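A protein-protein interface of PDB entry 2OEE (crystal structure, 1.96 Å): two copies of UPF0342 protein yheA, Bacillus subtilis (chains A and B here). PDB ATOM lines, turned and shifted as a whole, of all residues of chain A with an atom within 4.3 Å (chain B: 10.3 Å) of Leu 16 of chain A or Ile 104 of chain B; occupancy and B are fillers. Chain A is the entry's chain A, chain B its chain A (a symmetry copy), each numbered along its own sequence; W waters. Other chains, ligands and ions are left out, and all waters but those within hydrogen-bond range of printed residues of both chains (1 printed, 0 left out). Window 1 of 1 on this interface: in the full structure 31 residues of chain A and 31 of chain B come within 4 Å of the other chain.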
ATOM      1  N   ALA A   9       6.702 -17.207  34.509  1.00  0.00           N
ATOM      2  CA  ALA A   9       6.834 -17.448  33.066  1.00  0.00           C
ATOM      3  C   ALA A   9       5.461 -17.721  32.425  1.00  0.00           C
ATOM      4  O   ALA A   9       5.194 -17.241  31.322  1.00  0.00           O
ATOM      5  CB  ALA A   9       7.777 -18.592  32.788  1.00  0.00           C
ATOM      6  N   LEU A  12       3.701 -14.593  32.101  1.00  0.00           N
ATOM      7  CA  LEU A  12       4.274 -13.833  30.987  1.00  0.00           C
ATOM      8  C   LEU A  12       3.762 -14.346  29.651  1.00  0.00           C
ATOM      9  O   LEU A  12       3.453 -13.549  28.767  1.00  0.00           O
ATOM     10  CB  LEU A  12       5.812 -13.838  31.052  1.00  0.00           C
ATOM     11  CG  LEU A  12       6.553 -12.989  30.002  1.00  0.00           C
ATOM     12  CD1 LEU A  12       6.202 -11.493  30.106  1.00  0.00           C
ATOM     13  CD2 LEU A  12       8.088 -13.240  30.129  1.00  0.00           C
ATOM     14  N   GLU A  13       3.647 -15.669  29.505  1.00  0.00           N
ATOM     15  CA  GLU A  13       2.988 -16.259  28.326  1.00  0.00           C
ATOM     16  C   GLU A  13       1.568 -15.674  28.132  1.00  0.00           C
ATOM     17  O   GLU A  13       1.184 -15.274  27.007  1.00  0.00           O
ATOM     18  CB  GLU A  13       2.927 -17.799  28.458  1.00  0.00           C
ATOM     19  CG  GLU A  13       2.252 -18.494  27.290  1.00  0.00           C
ATOM     20  CD  GLU A  13       1.937 -19.949  27.550  1.00  0.00           C
ATOM     21  OE1 GLU A  13       2.140 -20.412  28.692  1.00  0.00           O
ATOM     22  OE2 GLU A  13       1.473 -20.640  26.596  1.00  0.00           O
ATOM     23  N   ASN A  14       0.812 -15.587  29.225  1.00  0.00           N
ATOM     24  CA  ASN A  14      -0.533 -15.019  29.190  1.00  0.00           C
ATOM     25  C   ASN A  14      -0.513 -13.557  28.773  1.00  0.00           C
ATOM     26  O   ASN A  14      -1.355 -13.137  27.980  1.00  0.00           O
ATOM     27  CB  ASN A  14      -1.255 -15.151  30.530  1.00  0.00           C
ATOM     28  CG  ASN A  14      -1.889 -16.525  30.737  1.00  0.00           C
ATOM     29  OD1 ASN A  14      -2.197 -16.906  31.872  1.00  0.00           O
ATOM     30  ND2 ASN A  14      -2.108 -17.254  29.659  1.00  0.00           N
ATOM     31  N   ALA A  15       0.434 -12.793  29.307  1.00  0.00           N
ATOM     32  CA  ALA A  15       0.594 -11.388  28.924  1.00  0.00           C
ATOM     33  C   ALA A  15       0.833 -11.260  27.417  1.00  0.00           C
ATOM     34  O   ALA A  15       0.222 -10.412  26.752  1.00  0.00           O
ATOM     35  CB  ALA A  15       1.749 -10.750  29.700  1.00  0.00           C
ATOM     36  N   LEU A  16       1.718 -12.098  26.887  1.00  0.00           N
ATOM     37  CA  LEU A  16       1.979 -12.117  25.442  1.00  0.00           C
ATOM     38  C   LEU A  16       0.743 -12.526  24.639  1.00  0.00           C
ATOM     39  O   LEU A  16       0.365 -11.842  23.659  1.00  0.00           O
ATOM     40  CB  LEU A  16       3.150 -13.025  25.101  1.00  0.00           C
ATOM     41  CG  LEU A  16       3.554 -12.988  23.619  1.00  0.00           C
ATOM     42  CD1 LEU A  16       3.979 -11.556  23.185  1.00  0.00           C
ATOM     43  CD2 LEU A  16       4.674 -13.994  23.357  1.00  0.00           C
ATOM     44  N   ARG A  17       0.105 -13.613  25.051  1.00  0.00           N
ATOM     45  CA  ARG A  17      -1.149 -14.065  24.392  1.00  0.00           C
ATOM     46  C   ARG A  17      -2.214 -12.978  24.293  1.00  0.00           C
ATOM     47  O   ARG A  17      -2.931 -12.901  23.299  1.00  0.00           O
ATOM     48  CB  ARG A  17      -1.756 -15.274  25.102  1.00  0.00           C
ATOM     49  CG  ARG A  17      -1.064 -16.572  24.789  1.00  0.00           C
ATOM     50  CD  ARG A  17      -1.729 -17.746  25.518  1.00  0.00           C
ATOM     51  NE  ARG A  17      -0.923 -18.940  25.360  1.00  0.00           N
ATOM     52  CZ  ARG A  17      -0.968 -19.736  24.300  1.00  0.00           C
ATOM     53  NH1 ARG A  17      -1.814 -19.483  23.297  1.00  0.00           N
ATOM     54  NH2 ARG A  17      -0.171 -20.785  24.240  1.00  0.00           N
ATOM     55  N   GLY A  18      -2.317 -12.163  25.340  1.00  0.00           N
ATOM     56  CA  GLY A  18      -3.346 -11.152  25.441  1.00  0.00           C
ATOM     57  C   GLY A  18      -2.933  -9.799  24.910  1.00  0.00           C
ATOM     58  O   GLY A  18      -3.732  -8.863  24.960  1.00  0.00           O
ATOM     59  N   SER A  19      -1.700  -9.674  24.416  1.00  0.00           N
ATOM     60  CA  SER A  19      -1.199  -8.380  24.007  1.00  0.00           C
ATOM     61  C   SER A  19      -1.759  -7.958  22.632  1.00  0.00           C
ATOM     62  O   SER A  19      -2.057  -8.797  21.768  1.00  0.00           O
ATOM     63  CB  SER A  19       0.329  -8.361  23.983  1.00  0.00           C
ATOM     64  OG  SER A  19       0.829  -9.232  22.975  1.00  0.00           O
ATOM     65  N   PHE A  22       0.559  -9.296  19.823  1.00  0.00           N
ATOM     66  CA  PHE A  22       0.291 -10.633  19.333  1.00  0.00           C
ATOM     67  C   PHE A  22      -0.921 -10.616  18.393  1.00  0.00           C
ATOM     68  O   PHE A  22      -0.902 -11.269  17.345  1.00  0.00           O
ATOM     69  CB  PHE A  22       0.062 -11.660  20.471  1.00  0.00           C
ATOM     70  CG  PHE A  22      -0.244 -13.026  19.947  1.00  0.00           C
ATOM     71  CD1 PHE A  22       0.773 -13.829  19.458  1.00  0.00           C
ATOM     72  CD2 PHE A  22      -1.559 -13.473  19.850  1.00  0.00           C
ATOM     73  CE1 PHE A  22       0.495 -15.086  18.906  1.00  0.00           C
ATOM     74  CE2 PHE A  22      -1.848 -14.723  19.295  1.00  0.00           C
ATOM     75  CZ  PHE A  22      -0.808 -15.530  18.821  1.00  0.00           C
ATOM     76  N   MET A  93       8.369  -8.595  17.029  1.00  0.00           N
ATOM     77  CA  MET A  93       8.138  -9.660  18.029  1.00  0.00           C
ATOM     78  C   MET A  93       9.483 -10.254  18.478  1.00  0.00           C
ATOM     79  O   MET A  93       9.706 -10.500  19.671  1.00  0.00           O
ATOM     80  CB  MET A  93       7.204 -10.763  17.498  1.00  0.00           C
ATOM     81  CG  MET A  93       6.848 -11.854  18.568  1.00  0.00           C
ATOM     82  SD  MET A  93       5.979 -11.203  20.044  1.00  0.00           S
ATOM     83  CE  MET A  93       4.419 -10.664  19.364  1.00  0.00           C
ATOM     84  N   LEU A  96      11.025  -7.834  20.802  1.00  0.00           N
ATOM     85  CA  LEU A  96      10.335  -7.890  22.105  1.00  0.00           C
ATOM     86  C   LEU A  96      10.863  -9.048  22.967  1.00  0.00           C
ATOM     87  O   LEU A  96      11.178  -8.866  24.153  1.00  0.00           O
ATOM     88  CB  LEU A  96       8.811  -7.998  21.946  1.00  0.00           C
ATOM     89  CG  LEU A  96       7.936  -8.211  23.202  1.00  0.00           C
ATOM     90  CD1 LEU A  96       8.047  -7.051  24.138  1.00  0.00           C
ATOM     91  CD2 LEU A  96       6.465  -8.400  22.830  1.00  0.00           C
ATOM     92  N   ILE A  97      10.981 -10.231  22.367  1.00  0.00           N
ATOM     93  CA  ILE A  97      11.518 -11.386  23.077  1.00  0.00           C
ATOM     94  C   ILE A  97      12.965 -11.096  23.526  1.00  0.00           C
ATOM     95  O   ILE A  97      13.364 -11.432  24.648  1.00  0.00           O
ATOM     96  CB  ILE A  97      11.435 -12.684  22.229  1.00  0.00           C
ATOM     97  CG1 ILE A  97       9.971 -13.025  21.917  1.00  0.00           C
ATOM     98  CG2 ILE A  97      12.121 -13.865  22.952  1.00  0.00           C
ATOM     99  CD1 ILE A  97       9.037 -13.078  23.128  1.00  0.00           C
ATOM    100  N   VAL B   3      -2.428  -8.444  31.679  1.00  0.00           N
ATOM    101  CA  VAL B   3      -1.336  -7.654  32.340  1.00  0.00           C
ATOM    102  C   VAL B   3      -0.295  -7.225  31.324  1.00  0.00           C
ATOM    103  O   VAL B   3      -0.241  -7.776  30.213  1.00  0.00           O
ATOM    104  CB  VAL B   3      -0.636  -8.448  33.437  1.00  0.00           C
ATOM    105  CG1 VAL B   3      -1.463  -8.436  34.731  1.00  0.00           C
ATOM    106  CG2 VAL B   3      -0.383  -9.843  32.966  1.00  0.00           C
ATOM    107  N   ASN B   4       0.524  -6.246  31.707  1.00  0.00           N
ATOM    108  CA  ASN B   4       1.567  -5.769  30.832  1.00  0.00           C
ATOM    109  C   ASN B   4       2.764  -6.709  30.815  1.00  0.00           C
ATOM    110  O   ASN B   4       3.287  -7.103  31.849  1.00  0.00           O
ATOM    111  CB  ASN B   4       2.029  -4.371  31.209  1.00  0.00           C
ATOM    112  CG  ASN B   4       3.098  -3.861  30.270  1.00  0.00           C
ATOM    113  OD1 ASN B   4       4.295  -4.029  30.518  1.00  0.00           O
ATOM    114  ND2 ASN B   4       2.672  -3.254  29.167  1.00  0.00           N
ATOM    115  N   PHE B   5       3.198  -7.007  29.605  1.00  0.00           N
ATOM    116  CA  PHE B   5       4.300  -7.887  29.351  1.00  0.00           C
ATOM    117  C   PHE B   5       5.600  -7.475  30.099  1.00  0.00           C
ATOM    118  O   PHE B   5       6.337  -8.330  30.622  1.00  0.00           O
ATOM    119  CB  PHE B   5       4.511  -7.857  27.853  1.00  0.00           C
ATOM    120  CG  PHE B   5       5.451  -8.839  27.395  1.00  0.00           C
ATOM    121  CD1 PHE B   5       5.015 -10.111  27.073  1.00  0.00           C
ATOM    122  CD2 PHE B   5       6.780  -8.515  27.294  1.00  0.00           C
ATOM    123  CE1 PHE B   5       5.882 -11.068  26.642  1.00  0.00           C
ATOM    124  CE2 PHE B   5       7.677  -9.462  26.855  1.00  0.00           C
ATOM    125  CZ  PHE B   5       7.219 -10.762  26.525  1.00  0.00           C
ATOM    126  N   TYR B   6       5.880  -6.173  30.129  1.00  0.00           N
ATOM    127  CA  TYR B   6       7.056  -5.671  30.851  1.00  0.00           C
ATOM    128  C   TYR B   6       6.919  -5.754  32.359  1.00  0.00           C
ATOM    129  O   TYR B   6       7.875  -6.157  33.033  1.00  0.00           O
ATOM    130  CB  TYR B   6       7.468  -4.258  30.389  1.00  0.00           C
ATOM    131  CG  TYR B   6       7.815  -4.229  28.943  1.00  0.00           C
ATOM    132  CD1 TYR B   6       8.962  -4.852  28.463  1.00  0.00           C
ATOM    133  CD2 TYR B   6       6.967  -3.607  28.031  1.00  0.00           C
ATOM    134  CE1 TYR B   6       9.262  -4.836  27.102  1.00  0.00           C
ATOM    135  CE2 TYR B   6       7.260  -3.579  26.696  1.00  0.00           C
ATOM    136  CZ  TYR B   6       8.399  -4.185  26.232  1.00  0.00           C
ATOM    137  OH  TYR B   6       8.655  -4.141  24.877  1.00  0.00           O
ATOM    138  N   ASP B   7       5.746  -5.419  32.892  1.00  0.00           N
ATOM    139  CA  ASP B   7       5.456  -5.644  34.319  1.00  0.00           C
ATOM    140  C   ASP B   7       5.779  -7.080  34.745  1.00  0.00           C
ATOM    141  O   ASP B   7       6.428  -7.308  35.779  1.00  0.00           O
ATOM    142  CB  ASP B   7       3.976  -5.371  34.663  1.00  0.00           C
ATOM    143  CG  ASP B   7       3.589  -3.870  34.599  1.00  0.00           C
ATOM    144  OD1 ASP B   7       4.449  -2.996  34.785  1.00  0.00           O
ATOM    145  OD2 ASP B   7       2.401  -3.579  34.374  1.00  0.00           O
ATOM    146  N   VAL B   8       5.290  -8.053  33.974  1.00  0.00           N
ATOM    147  CA  VAL B   8       5.528  -9.460  34.305  1.00  0.00           C
ATOM    148  C   VAL B   8       7.003  -9.822  34.148  1.00  0.00           C
ATOM    149  O   VAL B   8       7.536 -10.554  34.982  1.00  0.00           O
ATOM    150  CB  VAL B   8       4.632 -10.422  33.491  1.00  0.00           C
ATOM    151  CG1 VAL B   8       4.855 -11.862  33.921  1.00  0.00           C
ATOM    152  CG2 VAL B   8       3.161 -10.067  33.672  1.00  0.00           C
ATOM    153  N   ALA B   9       7.647  -9.324  33.085  1.00  0.00           N
ATOM    154  CA  ALA B   9       9.077  -9.571  32.860  1.00  0.00           C
ATOM    155  C   ALA B   9       9.910  -9.129  34.077  1.00  0.00           C
ATOM    156  O   ALA B   9      10.856  -9.822  34.455  1.00  0.00           O
ATOM    157  CB  ALA B   9       9.563  -8.873  31.615  1.00  0.00           C
ATOM    158  N   LEU B  12       9.531 -11.588  36.685  1.00  0.00           N
ATOM    159  CA  LEU B  12      10.321 -12.775  36.344  1.00  0.00           C
ATOM    160  C   LEU B  12      11.793 -12.562  36.655  1.00  0.00           C
ATOM    161  O   LEU B  12      12.446 -13.467  37.172  1.00  0.00           O
ATOM    162  CB  LEU B  12      10.098 -13.180  34.876  1.00  0.00           C
ATOM    163  CG  LEU B  12      10.784 -14.475  34.404  1.00  0.00           C
ATOM    164  CD1 LEU B  12      10.303 -15.711  35.186  1.00  0.00           C
ATOM    165  CD2 LEU B  12      10.571 -14.638  32.865  1.00  0.00           C
ATOM    166  N   LEU B  96      17.650 -23.175  31.505  1.00  0.00           N
ATOM    167  CA  LEU B  96      16.495 -22.542  32.172  1.00  0.00           C
ATOM    168  C   LEU B  96      15.941 -21.376  31.338  1.00  0.00           C
ATOM    169  O   LEU B  96      14.725 -21.276  31.113  1.00  0.00           O
ATOM    170  CB  LEU B  96      16.839 -22.065  33.591  1.00  0.00           C
ATOM    171  CG  LEU B  96      15.792 -21.251  34.384  1.00  0.00           C
ATOM    172  CD1 LEU B  96      14.562 -22.061  34.642  1.00  0.00           C
ATOM    173  CD2 LEU B  96      16.354 -20.778  35.726  1.00  0.00           C
ATOM    174  N   ILE B  97      16.832 -20.509  30.860  1.00  0.00           N
ATOM    175  CA  ILE B  97      16.421 -19.392  30.017  1.00  0.00           C
ATOM    176  C   ILE B  97      15.758 -19.928  28.731  1.00  0.00           C
ATOM    177  O   ILE B  97      14.738 -19.398  28.270  1.00  0.00           O
ATOM    178  CB  ILE B  97      17.601 -18.437  29.693  1.00  0.00           C
ATOM    179  CG1 ILE B  97      18.149 -17.810  30.984  1.00  0.00           C
ATOM    180  CG2 ILE B  97      17.169 -17.336  28.701  1.00  0.00           C
ATOM    181  CD1 ILE B  97      17.106 -17.139  31.881  1.00  0.00           C
ATOM    182  N   GLY B  98      16.354 -20.967  28.161  1.00  0.00           N
ATOM    183  CA  GLY B  98      15.756 -21.684  27.037  1.00  0.00           C
ATOM    184  C   GLY B  98      14.338 -22.169  27.330  1.00  0.00           C
ATOM    185  O   GLY B  98      13.460 -21.957  26.512  1.00  0.00           O
ATOM    186  N   GLU B  99      14.120 -22.801  28.488  1.00  0.00           N
ATOM    187  CA  GLU B  99      12.779 -23.241  28.908  1.00  0.00           C
ATOM    188  C   GLU B  99      11.806 -22.064  29.011  1.00  0.00           C
ATOM    189  O   GLU B  99      10.673 -22.130  28.539  1.00  0.00           O
ATOM    190  CB  GLU B  99      12.820 -23.972  30.256  1.00  0.00           C
ATOM    191  CG  GLU B  99      13.404 -25.371  30.190  1.00  0.00           C
ATOM    192  CD  GLU B  99      12.783 -26.189  29.071  1.00  0.00           C
ATOM    193  OE1 GLU B  99      11.556 -26.434  29.119  1.00  0.00           O
ATOM    194  OE2 GLU B  99      13.522 -26.567  28.135  1.00  0.00           O
ATOM    195  N   LEU B 100      12.251 -20.976  29.621  1.00  0.00           N
ATOM    196  CA  LEU B 100      11.372 -19.824  29.756  1.00  0.00           C
ATOM    197  C   LEU B 100      10.951 -19.315  28.409  1.00  0.00           C
ATOM    198  O   LEU B 100       9.764 -19.024  28.215  1.00  0.00           O
ATOM    199  CB  LEU B 100      12.046 -18.726  30.565  1.00  0.00           C
ATOM    200  CG  LEU B 100      12.423 -19.350  31.896  1.00  0.00           C
ATOM    201  CD1 LEU B 100      13.127 -18.280  32.657  1.00  0.00           C
ATOM    202  CD2 LEU B 100      11.193 -19.951  32.680  1.00  0.00           C
ATOM    203  N   ASN B 101      11.900 -19.259  27.476  1.00  0.00           N
ATOM    204  CA  ASN B 101      11.645 -18.830  26.092  1.00  0.00           C
ATOM    205  C   ASN B 101      10.653 -19.733  25.351  1.00  0.00           C
ATOM    206  O   ASN B 101       9.687 -19.237  24.776  1.00  0.00           O
ATOM    207  CB  ASN B 101      12.943 -18.637  25.304  1.00  0.00           C
ATOM    208  CG  ASN B 101      13.596 -17.265  25.581  1.00  0.00           C
ATOM    209  OD1 ASN B 101      13.174 -16.264  25.047  1.00  0.00           O
ATOM    210  ND2 ASN B 101      14.574 -17.228  26.471  1.00  0.00           N
ATOM    211  N   LYS B 102      10.875 -21.046  25.397  1.00  0.00           N
ATOM    212  CA  LYS B 102       9.885 -21.998  24.891  1.00  0.00           C
ATOM    213  C   LYS B 102       8.479 -21.813  25.493  1.00  0.00           C
ATOM    214  O   LYS B 102       7.481 -21.931  24.781  1.00  0.00           O
ATOM    215  CB  LYS B 102      10.346 -23.423  25.143  1.00  0.00           C
ATOM    216  CG  LYS B 102      11.515 -23.853  24.288  1.00  0.00           C
ATOM    217  CD  LYS B 102      11.909 -25.302  24.598  1.00  0.00           C
ATOM    218  CE  LYS B 102      10.822 -26.290  24.164  1.00  0.00           C
ATOM    219  NZ  LYS B 102      10.688 -26.381  22.665  1.00  0.00           N
ATOM    220  N   ILE B 103       8.396 -21.583  26.799  1.00  0.00           N
ATOM    221  CA  ILE B 103       7.099 -21.337  27.451  1.00  0.00           C
ATOM    222  C   ILE B 103       6.391 -20.111  26.853  1.00  0.00           C
ATOM    223  O   ILE B 103       5.266 -20.206  26.354  1.00  0.00           O
ATOM    224  CB  ILE B 103       7.257 -21.175  28.985  1.00  0.00           C
ATOM    225  CG1 ILE B 103       7.577 -22.538  29.619  1.00  0.00           C
ATOM    226  CG2 ILE B 103       6.003 -20.515  29.627  1.00  0.00           C
ATOM    227  CD1 ILE B 103       7.886 -22.488  31.116  1.00  0.00           C
ATOM    228  N   ILE B 104       7.070 -18.974  26.882  1.00  0.00           N
ATOM    229  CA  ILE B 104       6.447 -17.702  26.495  1.00  0.00           C
ATOM    230  C   ILE B 104       6.206 -17.595  24.993  1.00  0.00           C
ATOM    231  O   ILE B 104       5.305 -16.864  24.556  1.00  0.00           O
ATOM    232  CB  ILE B 104       7.269 -16.490  26.982  1.00  0.00           C
ATOM    233  CG1 ILE B 104       8.593 -16.405  26.214  1.00  0.00           C
ATOM    234  CG2 ILE B 104       7.448 -16.553  28.496  1.00  0.00           C
ATOM    235  CD1 ILE B 104       9.334 -15.070  26.339  1.00  0.00           C
ATOM    236  N   MET B 105       6.991 -18.323  24.207  1.00  0.00           N
ATOM    237  CA  MET B 105       6.878 -18.291  22.752  1.00  0.00           C
ATOM    238  C   MET B 105       5.876 -19.309  22.162  1.00  0.00           C
ATOM    239  O   MET B 105       5.677 -19.363  20.943  1.00  0.00           O
ATOM    240  CB  MET B 105       8.256 -18.438  22.096  1.00  0.00           C
ATOM    241  CG  MET B 105       9.215 -17.252  22.399  1.00  0.00           C
ATOM    242  SD  MET B 105      10.828 -17.440  21.605  1.00  0.00           S
ATOM    243  CE  MET B 105      10.332 -17.328  19.876  1.00  0.00           C
ATOM    244  N   LYS B 106       5.251 -20.102  23.033  1.00  0.00           N
ATOM    245  CA  LYS B 106       4.216 -21.065  22.621  1.00  0.00           C
ATOM    246  C   LYS B 106       3.122 -20.459  21.716  1.00  0.00           C
ATOM    247  O   LYS B 106       2.752 -21.079  20.717  1.00  0.00           O
ATOM    248  CB  LYS B 106       3.529 -21.652  23.841  1.00  0.00           C
ATOM    249  CG  LYS B 106       3.202 -23.109  23.725  1.00  0.00           C
ATOM    250  CD  LYS B 106       4.093 -23.870  24.715  1.00  0.00           C
ATOM    251  CE  LYS B 106       5.431 -24.278  24.138  1.00  0.00           C
ATOM    252  NZ  LYS B 106       5.441 -25.695  23.683  1.00  0.00           N
ATOM    253  N   PRO B 107       2.564 -19.295  22.101  1.00  0.00           N
ATOM    254  CA  PRO B 107       1.570 -18.678  21.198  1.00  0.00           C
ATOM    255  C   PRO B 107       2.083 -18.419  19.771  1.00  0.00           C
ATOM    256  O   PRO B 107       1.305 -18.526  18.818  1.00  0.00           O
ATOM    257  CB  PRO B 107       1.153 -17.394  21.922  1.00  0.00           C
ATOM    258  CG  PRO B 107       2.147 -17.197  23.029  1.00  0.00           C
ATOM    259  CD  PRO B 107       2.699 -18.541  23.362  1.00  0.00           C
ATOM    260  N   LEU B 108       3.378 -18.149  19.617  1.00  0.00           N
ATOM    261  CA  LEU B 108       3.987 -17.970  18.284  1.00  0.00           C
ATOM    262  C   LEU B 108       4.076 -19.292  17.504  1.00  0.00           C
ATOM    263  O   LEU B 108       3.735 -19.365  16.327  1.00  0.00           O
ATOM    264  CB  LEU B 108       5.364 -17.287  18.403  1.00  0.00           C
ATOM    265  CG  LEU B 108       5.293 -15.944  19.144  1.00  0.00           C
ATOM    266  CD1 LEU B 108       6.674 -15.335  19.464  1.00  0.00           C
ATOM    267  CD2 LEU B 108       4.402 -14.955  18.363  1.00  0.00           C
ATOM    268  N   GLU B 109       4.520 -20.336  18.188  1.00  0.00           N
ATOM    269  CA  GLU B 109       4.557 -21.683  17.635  1.00  0.00           C
ATOM    270  C   GLU B 109       3.152 -22.146  17.182  1.00  0.00           C
ATOM    271  O   GLU B 109       3.013 -22.715  16.098  1.00  0.00           O
ATOM    272  CB  GLU B 109       5.194 -22.624  18.670  1.00  0.00           C
ATOM    273  CG  GLU B 109       5.115 -24.103  18.368  1.00  0.00           C
ATOM    274  CD  GLU B 109       5.849 -24.928  19.414  1.00  0.00           C
ATOM    275  OE1 GLU B 109       6.961 -24.504  19.830  1.00  0.00           O
ATOM    276  OE2 GLU B 109       5.313 -25.990  19.818  1.00  0.00           O
ATOM    277  N   GLU B 110       2.121 -21.874  17.985  1.00  0.00           N
ATOM    278  CA  GLU B 110       0.737 -22.179  17.604  1.00  0.00           C
ATOM    279  C   GLU B 110       0.358 -21.456  16.298  1.00  0.00           C
ATOM    280  O   GLU B 110      -0.245 -22.041  15.399  1.00  0.00           O
ATOM    281  CB  GLU B 110      -0.235 -21.793  18.728  1.00  0.00           C
ATOM    282  CG  GLU B 110      -0.150 -22.690  19.957  1.00  0.00           C
ATOM    283  CD  GLU B 110      -0.804 -22.091  21.181  1.00  0.00           C
ATOM    284  OE1 GLU B 110      -1.530 -21.063  21.057  1.00  0.00           O
ATOM    285  OE2 GLU B 110      -0.596 -22.653  22.290  1.00  0.00           O
ATOM    286  N   LEU B 111       0.744 -20.188  16.196  1.00  0.00           N
ATOM    287  CA  LEU B 111       0.409 -19.369  15.035  1.00  0.00           C
ATOM    288  C   LEU B 111       0.999 -19.908  13.730  1.00  0.00           C
ATOM    289  O   LEU B 111       0.299 -19.972  12.730  1.00  0.00           O
ATOM    290  CB  LEU B 111       0.833 -17.915  15.261  1.00  0.00           C
ATOM    291  CG  LEU B 111       0.519 -16.874  14.184  1.00  0.00           C
ATOM    292  CD1 LEU B 111      -0.990 -16.800  13.914  1.00  0.00           C
ATOM    293  CD2 LEU B 111       1.060 -15.506  14.624  1.00  0.00           C
HETATM  294  O   HOH W   1      -0.854  -8.283  27.549  1.00  0.00           O
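NH2 of Arg 17 of chain A lies within salt-bridge range of OE2 of Glu 110 of chain B, 2.7 Å away.
The side-chain hydroxyl (OG) of Ser 19 of chain A sits at hydrogen-bond distance from the backbone NH (N) of Phe 22 of chain A (3.2 Å). The side-chain amino group (NZ) of Lys 106 of chain B is in salt-bridge range of the side-chain carboxylate (OE2) of Glu 109 of chain B, 3.9 Å away. The backbone carbonyl oxygen (O) of Ile 97 of chain B lies within hydrogen-bond range of the side-chain amide nitrogen (ND2) of Asn 101 of chain B. The side-chain amide oxygen (OD1) of Asn 4 of chain B is in hydrogen-bond range of the backbone NH (N) of Tyr 6 of chain B (2.7 Å). The backbone carbonyl oxygen (O) of Leu 16 of chain A is in hydrogen-bond range of the side-chain hydroxyl (OG) of Ser 19 of chain A (2.7 Å). The side-chain carboxylate of Glu 13 of chain A lies within salt-bridge range of the guanidinium group of Arg 17 of chain A, 2.9 Å away.
Among the printed residues, pairs that only touch across the chains: Ala 9 of chain A with Leu 12 of chain B, Ala 9 of chain A with Leu 100 of chain B, Ala 9 of chain A with Ile 103 of chain B, Ala 9 of chain A with Ile 104 of chain B, Leu 12 of chain A with Phe 5 of chain B, Leu 12 of chain A with Val 8 of chain B, Leu 12 of chain A with Ala 9 of chain B, Leu 12 of chain A with Leu 12 of chain B, Leu 12 of chain A with Ile 104 of chain B, Glu 13 of chain A with Ile 103 of chain B, Glu 13 of chain A with Lys 106 of chain B, Glu 13 of chain A with Pro 107 of chain B, Ala 15 of chain A with Val 3 of chain B, Ala 15 of chain A with Phe 5 of chain B, Leu 16 of chain A with Phe 5 of chain B, Leu 16 of chain A with Ile 104 of chain B, Arg 17 of chain A with Lys 106 of chain B, Arg 17 of chain A with Pro 107 of chain B, Phe 22 of chain A with Pro 107 of chain B, Phe 22 of chain A with Leu 108 of chain B, Met 93 of chain A with Leu 108 of chain B, Leu 96 of chain A with Phe 5 of chain B, Leu 96 of chain A with Tyr 6 of chain B, Ile 97 of chain A with Asn 101 of chain B and Ile 97 of chain A with Ile 104 of chain B.
Of chain B, only Phe 5 and Ile 104 come within 4 Å of Leu 16 of chain A. Ile 104 of chain B touches four residues of chain A. Ala 9 of chain A touches four residues of chain B. Of chain B, only Val 3 (3.6 Å) and Phe 5 (3.9 Å) come within 4 Å of Ala 15 of chain A. No residue of chain B comes within 4 Å of Gly 18 of chain A. No residue of chain B comes within 4 Å of Ser 19 of chain A. Of the printed residues of chain B, Met 93 of chain A touches Leu 108. Printed residues of chain A within 4 Å of Val 8 of chain B: Leu 12. Of the printed residues of chain B, Leu 96 of chain A touches Phe 5 (3.7 Å) and Tyr 6 (3.1 Å). Printed residues of chain A within 4 Å of Leu 12 of chain B: Ala 9 (3.96 Å) and Leu 12 (3.95 Å). Printed residues of chain A within 4 Å of Ala 9 of chain B: Leu 12 (3.96 Å). The nearest residue of chain A that does not touch Ile 104 of chain B is Glu 13 of chain A (4.03 Å). The nearest printed residue of chain A that does not touch Phe 5 of chain B is Ile 97 of chain A (4.5 Å).
Of the 24 printed residues of chain B, 14 touch a printed residue of chain A. Hydrophobic or aromatic side chains of chain B within 4 Å of the printed part of chain A: Phe 5, Tyr 6, Val 8, Leu 12, Leu 100, Ile 103, Ile 104, Pro 107 and Leu 108. Hydrophobic or aromatic side chains of chain A that line the printed part of chain B: Ala 9, Leu 12, Ala 15, Leu 16, Phe 22, Met 93, Leu 96 and Ile 97. Among the printed residues, 26 pairs touch across the chains. Among the printed residues, Asp or Glu carboxylates within 4 Å of a Lys or Arg side-chain nitrogen of the other chain: Arg 17 of chain A with Glu 110 of chain B (2.7 Å).
Ala 9 of chain A touches Leu 12 of chain B, and with the chains exchanged Leu 12 of chain A touches Ala 9 of chain B. Leu 12 of chain B touches its own counterpart, Leu 12 of chain A. Of the 26 pairs that touch across the chains among the printed residues, 3 have their exchanged pair printed and touching as well.
Water W1 bridges O of Ala 15 of chain A (2.5 Å) and O of Val 3 of chain B (2.8 Å).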
